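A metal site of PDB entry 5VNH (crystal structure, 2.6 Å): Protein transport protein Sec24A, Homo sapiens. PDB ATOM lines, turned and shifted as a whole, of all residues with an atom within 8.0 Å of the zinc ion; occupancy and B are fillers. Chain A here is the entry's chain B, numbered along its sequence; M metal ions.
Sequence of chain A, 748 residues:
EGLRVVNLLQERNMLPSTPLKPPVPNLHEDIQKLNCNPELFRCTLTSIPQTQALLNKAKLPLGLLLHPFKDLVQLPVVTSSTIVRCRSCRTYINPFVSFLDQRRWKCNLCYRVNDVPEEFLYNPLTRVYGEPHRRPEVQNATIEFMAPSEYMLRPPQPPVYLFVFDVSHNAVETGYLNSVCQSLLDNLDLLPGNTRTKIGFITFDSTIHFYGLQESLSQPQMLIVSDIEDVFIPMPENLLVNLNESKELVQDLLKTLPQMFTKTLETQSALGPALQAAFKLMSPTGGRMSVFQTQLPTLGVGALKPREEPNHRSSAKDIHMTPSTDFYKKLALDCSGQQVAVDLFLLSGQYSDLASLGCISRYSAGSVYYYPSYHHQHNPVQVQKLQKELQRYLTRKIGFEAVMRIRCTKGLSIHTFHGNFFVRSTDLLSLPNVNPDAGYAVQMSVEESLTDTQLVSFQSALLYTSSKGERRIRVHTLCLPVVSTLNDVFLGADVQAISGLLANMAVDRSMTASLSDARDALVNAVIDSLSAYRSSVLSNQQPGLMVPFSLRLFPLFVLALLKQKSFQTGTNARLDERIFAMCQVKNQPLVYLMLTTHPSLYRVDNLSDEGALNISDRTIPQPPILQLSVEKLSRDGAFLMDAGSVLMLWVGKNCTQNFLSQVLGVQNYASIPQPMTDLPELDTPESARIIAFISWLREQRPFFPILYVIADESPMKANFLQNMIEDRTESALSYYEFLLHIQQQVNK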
ATOM      1  N   ARG A  85      14.179  31.616  28.686  1.00  0.00           N
ATOM      2  CA  ARG A  85      14.000  30.170  28.574  1.00  0.00           C
ATOM      3  C   ARG A  85      15.235  29.565  27.906  1.00  0.00           C
ATOM      4  O   ARG A  85      15.950  30.239  27.170  1.00  0.00           O
ATOM      5  CB  ARG A  85      12.744  29.810  27.761  1.00  0.00           C
ATOM      6  CG  ARG A  85      11.455  30.326  28.366  1.00  0.00           C
ATOM      7  CD  ARG A  85      10.265  30.062  27.460  1.00  0.00           C
ATOM      8  NE  ARG A  85       9.862  28.653  27.445  1.00  0.00           N
ATOM      9  CZ  ARG A  85       8.791  28.192  26.822  1.00  0.00           C
ATOM     10  NH1 ARG A  85       8.003  29.024  26.153  1.00  0.00           N
ATOM     11  NH2 ARG A  85       8.502  26.895  26.855  1.00  0.00           N
ATOM     12  N   CYS A  86      15.456  28.277  28.177  1.00  0.00           N
ATOM     13  CA  CYS A  86      16.549  27.579  27.530  1.00  0.00           C
ATOM     14  C   CYS A  86      16.314  27.499  26.030  1.00  0.00           C
ATOM     15  O   CYS A  86      15.180  27.288  25.576  1.00  0.00           O
ATOM     16  CB  CYS A  86      16.695  26.170  28.120  1.00  0.00           C
ATOM     17  SG  CYS A  86      17.964  25.153  27.325  1.00  0.00           S
ATOM     18  N   ARG A  87      17.381  27.688  25.247  1.00  0.00           N
ATOM     19  CA  ARG A  87      17.266  27.705  23.797  1.00  0.00           C
ATOM     20  C   ARG A  87      17.031  26.323  23.192  1.00  0.00           C
ATOM     21  O   ARG A  87      16.737  26.230  21.996  1.00  0.00           O
ATOM     22  CB  ARG A  87      18.508  28.326  23.176  1.00  0.00           C
ATOM     23  CG  ARG A  87      18.625  29.828  23.344  1.00  0.00           C
ATOM     24  CD  ARG A  87      19.897  30.345  22.701  1.00  0.00           C
ATOM     25  NE  ARG A  87      20.007  31.798  22.720  1.00  0.00           N
ATOM     26  CZ  ARG A  87      21.056  32.478  22.273  1.00  0.00           C
ATOM     27  NH1 ARG A  87      22.093  31.823  21.755  1.00  0.00           N
ATOM     28  NH2 ARG A  87      21.067  33.793  22.332  1.00  0.00           N
ATOM     29  N   SER A  88      17.157  25.249  23.980  1.00  0.00           N
ATOM     30  CA  SER A  88      17.026  23.890  23.468  1.00  0.00           C
ATOM     31  C   SER A  88      15.709  23.233  23.886  1.00  0.00           C
ATOM     32  O   SER A  88      14.904  22.864  23.025  1.00  0.00           O
ATOM     33  CB  SER A  88      18.204  23.023  23.924  1.00  0.00           C
ATOM     34  OG  SER A  88      19.357  23.290  23.139  1.00  0.00           O
ATOM     35  N   CYS A  89      15.471  23.063  25.177  1.00  0.00           N
ATOM     36  CA  CYS A  89      14.263  22.398  25.670  1.00  0.00           C
ATOM     37  C   CYS A  89      13.193  23.378  26.133  1.00  0.00           C
ATOM     38  O   CYS A  89      12.164  22.944  26.662  1.00  0.00           O
ATOM     39  CB  CYS A  89      14.614  21.432  26.809  1.00  0.00           C
ATOM     40  SG  CYS A  89      15.282  22.242  28.273  1.00  0.00           S
ATOM     41  N   ARG A  90      13.418  24.676  25.960  1.00  0.00           N
ATOM     42  CA  ARG A  90      12.466  25.730  26.315  1.00  0.00           C
ATOM     43  C   ARG A  90      12.120  25.736  27.797  1.00  0.00           C
ATOM     44  O   ARG A  90      11.064  26.238  28.192  1.00  0.00           O
ATOM     45  CB  ARG A  90      11.180  25.616  25.484  1.00  0.00           C
ATOM     46  CG  ARG A  90      11.397  25.466  23.984  1.00  0.00           C
ATOM     47  CD  ARG A  90      12.314  26.552  23.420  1.00  0.00           C
ATOM     48  NE  ARG A  90      11.976  27.878  23.937  1.00  0.00           N
ATOM     49  CZ  ARG A  90      10.974  28.626  23.482  1.00  0.00           C
ATOM     50  NH1 ARG A  90      10.196  28.183  22.512  1.00  0.00           N
ATOM     51  NH2 ARG A  90      10.755  29.821  24.009  1.00  0.00           N
ATOM     52  N   THR A  91      12.996  25.192  28.642  1.00  0.00           N
ATOM     53  CA  THR A  91      12.763  25.209  30.075  1.00  0.00           C
ATOM     54  C   THR A  91      12.892  26.632  30.609  1.00  0.00           C
ATOM     55  O   THR A  91      13.869  27.329  30.312  1.00  0.00           O
ATOM     56  CB  THR A  91      13.751  24.285  30.791  1.00  0.00           C
ATOM     57  OG1 THR A  91      13.598  22.945  30.291  1.00  0.00           O
ATOM     58  CG2 THR A  91      13.496  24.286  32.285  1.00  0.00           C
ATOM     59  N   TYR A  92      11.912  27.057  31.397  1.00  0.00           N
ATOM     60  CA  TYR A  92      11.966  28.374  32.007  1.00  0.00           C
ATOM     61  C   TYR A  92      13.077  28.422  33.046  1.00  0.00           C
ATOM     62  O   TYR A  92      13.301  27.467  33.784  1.00  0.00           O
ATOM     63  CB  TYR A  92      10.625  28.725  32.656  1.00  0.00           C
ATOM     64  CG  TYR A  92       9.466  28.732  31.684  1.00  0.00           C
ATOM     65  CD1 TYR A  92       8.766  27.576  31.389  1.00  0.00           C
ATOM     66  CD2 TYR A  92       9.065  29.909  31.067  1.00  0.00           C
ATOM     67  CE1 TYR A  92       7.699  27.577  30.507  1.00  0.00           C
ATOM     68  CE2 TYR A  92       8.006  29.932  30.185  1.00  0.00           C
ATOM     69  CZ  TYR A  92       7.326  28.760  29.901  1.00  0.00           C
ATOM     70  OH  TYR A  92       6.267  28.777  29.027  1.00  0.00           O
ATOM     71  N   TRP A 105      24.103  30.750  31.816  1.00  0.00           N
ATOM     72  CA  TRP A 105      23.515  29.811  32.764  1.00  0.00           C
ATOM     73  C   TRP A 105      23.319  28.458  32.103  1.00  0.00           C
ATOM     74  O   TRP A 105      23.015  28.374  30.901  1.00  0.00           O
ATOM     75  CB  TRP A 105      22.172  30.324  33.305  1.00  0.00           C
ATOM     76  CG  TRP A 105      21.086  30.501  32.279  1.00  0.00           C
ATOM     77  CD1 TRP A 105      20.982  31.501  31.360  1.00  0.00           C
ATOM     78  CD2 TRP A 105      19.947  29.655  32.084  1.00  0.00           C
ATOM     79  NE1 TRP A 105      19.851  31.333  30.600  1.00  0.00           N
ATOM     80  CE2 TRP A 105      19.186  30.205  31.017  1.00  0.00           C
ATOM     81  CE3 TRP A 105      19.481  28.488  32.698  1.00  0.00           C
ATOM     82  CZ2 TRP A 105      18.007  29.623  30.567  1.00  0.00           C
ATOM     83  CZ3 TRP A 105      18.315  27.915  32.240  1.00  0.00           C
ATOM     84  CH2 TRP A 105      17.585  28.482  31.179  1.00  0.00           C
ATOM     85  N   LYS A 106      23.515  27.401  32.881  1.00  0.00           N
ATOM     86  CA  LYS A 106      23.347  26.029  32.412  1.00  0.00           C
ATOM     87  C   LYS A 106      21.950  25.537  32.753  1.00  0.00           C
ATOM     88  O   LYS A 106      21.539  25.592  33.917  1.00  0.00           O
ATOM     89  CB  LYS A 106      24.400  25.098  33.016  1.00  0.00           C
ATOM     90  CG  LYS A 106      24.196  23.628  32.668  1.00  0.00           C
ATOM     91  CD  LYS A 106      25.382  22.787  33.114  1.00  0.00           C
ATOM     92  CE  LYS A 106      26.648  23.175  32.358  1.00  0.00           C
ATOM     93  NZ  LYS A 106      27.817  22.378  32.806  1.00  0.00           N
ATOM     94  N   CYS A 107      21.226  25.057  31.747  1.00  0.00           N
ATOM     95  CA  CYS A 107      19.905  24.501  31.980  1.00  0.00           C
ATOM     96  C   CYS A 107      20.017  23.250  32.847  1.00  0.00           C
ATOM     97  O   CYS A 107      20.897  22.410  32.643  1.00  0.00           O
ATOM     98  CB  CYS A 107      19.240  24.171  30.640  1.00  0.00           C
ATOM     99  SG  CYS A 107      17.557  23.551  30.794  1.00  0.00           S
ATOM    100  N   ASN A 108      19.135  23.147  33.838  1.00  0.00           N
ATOM    101  CA  ASN A 108      19.147  22.024  34.758  1.00  0.00           C
ATOM    102  C   ASN A 108      18.331  20.838  34.265  1.00  0.00           C
ATOM    103  O   ASN A 108      18.157  19.860  35.007  1.00  0.00           O
ATOM    104  CB  ASN A 108      18.647  22.455  36.137  1.00  0.00           C
ATOM    105  CG  ASN A 108      17.343  23.224  36.060  1.00  0.00           C
ATOM    106  OD1 ASN A 108      17.097  23.950  35.104  1.00  0.00           O
ATOM    107  ND2 ASN A 108      16.501  23.064  37.075  1.00  0.00           N
ATOM    108  N   LEU A 109      17.829  20.898  33.032  1.00  0.00           N
ATOM    109  CA  LEU A 109      17.058  19.796  32.466  1.00  0.00           C
ATOM    110  C   LEU A 109      17.707  19.183  31.227  1.00  0.00           C
ATOM    111  O   LEU A 109      17.591  17.962  31.034  1.00  0.00           O
ATOM    112  CB  LEU A 109      15.633  20.270  32.112  1.00  0.00           C
ATOM    113  CG  LEU A 109      14.613  20.266  33.259  1.00  0.00           C
ATOM    114  CD1 LEU A 109      14.852  21.418  34.218  1.00  0.00           C
ATOM    115  CD2 LEU A 109      13.195  20.309  32.715  1.00  0.00           C
ATOM    116  N   CYS A 110      18.373  19.975  30.399  1.00  0.00           N
ATOM    117  CA  CYS A 110      19.067  19.455  29.226  1.00  0.00           C
ATOM    118  C   CYS A 110      20.548  19.781  29.198  1.00  0.00           C
ATOM    119  O   CYS A 110      21.231  19.410  28.240  1.00  0.00           O
ATOM    120  CB  CYS A 110      18.403  19.974  27.931  1.00  0.00           C
ATOM    121  SG  CYS A 110      18.873  21.656  27.470  1.00  0.00           S
ATOM    122  N   TYR A 111      21.055  20.496  30.211  1.00  0.00           N
ATOM    123  CA  TYR A 111      22.472  20.746  30.443  1.00  0.00           C
ATOM    124  C   TYR A 111      23.106  21.698  29.441  1.00  0.00           C
ATOM    125  O   TYR A 111      24.341  21.860  29.442  1.00  0.00           O
ATOM    126  CB  TYR A 111      23.289  19.441  30.491  1.00  0.00           C
ATOM    127  CG  TYR A 111      22.723  18.397  31.428  1.00  0.00           C
ATOM    128  CD1 TYR A 111      22.204  18.745  32.664  1.00  0.00           C
ATOM    129  CD2 TYR A 111      22.710  17.050  31.070  1.00  0.00           C
ATOM    130  CE1 TYR A 111      21.687  17.799  33.522  1.00  0.00           C
ATOM    131  CE2 TYR A 111      22.196  16.096  31.913  1.00  0.00           C
ATOM    132  CZ  TYR A 111      21.684  16.471  33.139  1.00  0.00           C
ATOM    133  OH  TYR A 111      21.176  15.520  33.994  1.00  0.00           O
ATOM    134  N   ARG A 112      22.323  22.330  28.566  1.00  0.00           N
ATOM    135  CA  ARG A 112      22.883  23.284  27.617  1.00  0.00           C
ATOM    136  C   ARG A 112      23.180  24.619  28.304  1.00  0.00           C
ATOM    137  O   ARG A 112      22.420  25.061  29.171  1.00  0.00           O
ATOM    138  CB  ARG A 112      21.938  23.505  26.442  1.00  0.00           C
ATOM    139  CG  ARG A 112      22.111  24.860  25.761  1.00  0.00           C
ATOM    140  CD  ARG A 112      21.802  24.857  24.285  1.00  0.00           C
ATOM    141  NE  ARG A 112      22.051  26.169  23.687  1.00  0.00           N
ATOM    142  CZ  ARG A 112      21.688  26.517  22.466  1.00  0.00           C
ATOM    143  NH1 ARG A 112      21.033  25.675  21.685  1.00  0.00           N
ATOM    144  NH2 ARG A 112      21.965  27.736  22.010  1.00  0.00           N
ATOM    145  N   VAL A 113      24.280  25.245  27.914  1.00  0.00           N
ATOM    146  CA  VAL A 113      24.625  26.578  28.392  1.00  0.00           C
ATOM    147  C   VAL A 113      23.879  27.610  27.562  1.00  0.00           C
ATOM    148  O   VAL A 113      23.894  27.567  26.329  1.00  0.00           O
ATOM    149  CB  VAL A 113      26.144  26.806  28.321  1.00  0.00           C
ATOM    150  CG1 VAL A 113      26.545  28.023  29.140  1.00  0.00           C
ATOM    151  CG2 VAL A 113      26.888  25.562  28.792  1.00  0.00           C
ATOM    152  N   ASN A 114      23.212  28.547  28.236  1.00  0.00           N
ATOM    153  CA  ASN A 114      22.447  29.592  27.585  1.00  0.00           C
ATOM    154  C   ASN A 114      23.006  30.962  27.949  1.00  0.00           C
ATOM    155  O   ASN A 114      23.670  31.135  28.970  1.00  0.00           O
ATOM    156  CB  ASN A 114      20.963  29.531  27.966  1.00  0.00           C
ATOM    157  CG  ASN A 114      20.277  28.320  27.380  1.00  0.00           C
ATOM    158  OD1 ASN A 114      19.909  28.304  26.208  1.00  0.00           O
ATOM    159  ND2 ASN A 114      20.075  27.295  28.201  1.00  0.00           N
ATOM    160  N   ARG A 407       7.974  19.186  32.108  1.00  0.00           N
ATOM    161  CA  ARG A 407       9.328  18.927  31.642  1.00  0.00           C
ATOM    162  C   ARG A 407      10.158  18.335  32.771  1.00  0.00           C
ATOM    163  O   ARG A 407      10.018  18.733  33.940  1.00  0.00           O
ATOM    164  CB  ARG A 407       9.993  20.207  31.135  1.00  0.00           C
ATOM    165  CG  ARG A 407       9.370  20.795  29.882  1.00  0.00           C
ATOM    166  CD  ARG A 407      10.162  22.006  29.406  1.00  0.00           C
ATOM    167  NE  ARG A 407       9.684  22.508  28.118  1.00  0.00           N
ATOM    168  CZ  ARG A 407       8.779  23.463  27.976  1.00  0.00           C
ATOM    169  NH1 ARG A 407       8.241  24.038  29.038  1.00  0.00           N
ATOM    170  NH2 ARG A 407       8.415  23.855  26.767  1.00  0.00           N
HETATM  171 ZN    ZN M   1      17.417  23.186  28.459  1.00  0.00          ZN
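SG of Cys 86 sits close to N of Ser 88 (3.4 Å).
The side-chain sulfur (SG) of Cys 107 lies close to the backbone NH (N) of Leu 109, at 3.5 Å.
The backbone carbonyl oxygen (O) of Thr 91 lies within hydrogen-bond range of the backbone NH (N) of Cys 86, at 2.8 Å.
The backbone carbonyl oxygen (O) of Arg 112 is in hydrogen-bond range of the backbone NH (N) of Cys 107 (2.8 Å).
The side-chain sulfur (SG) of Cys 89 lies close to the side-chain hydroxyl (OG1) of Thr 91.
NE of Arg 407 lies within hydrogen-bond range of O of Cys 89 (2.9 Å).
The side-chain sulfur (SG) of Cys 110 sits close to the backbone NH (N) of Arg 112 (3.7 Å).
SG of Cys 86 lies close to ND2 of Asn 114, 3.1 Å away.
The side-chain sulfur (SG) of Cys 110 binds the zinc ion (2.3 Å).
SG of Cys 86 is bound to the zinc ion.
The zinc ion is bound by the side-chain sulfur (SG) of Cys 89, at 2.3 Å.
SG of Cys 107 is bound to the zinc ion.
The zinc ion has four donor atoms within binding distance.
Of the 19 residues printed, 4 come within 4 Å of the zinc ion.
Along chain A the residues within 4 Å of the zinc ion span positions 86 to 110.
The nearest printed residue that does not touch the zinc ion is Thr 91 (4.2 Å).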
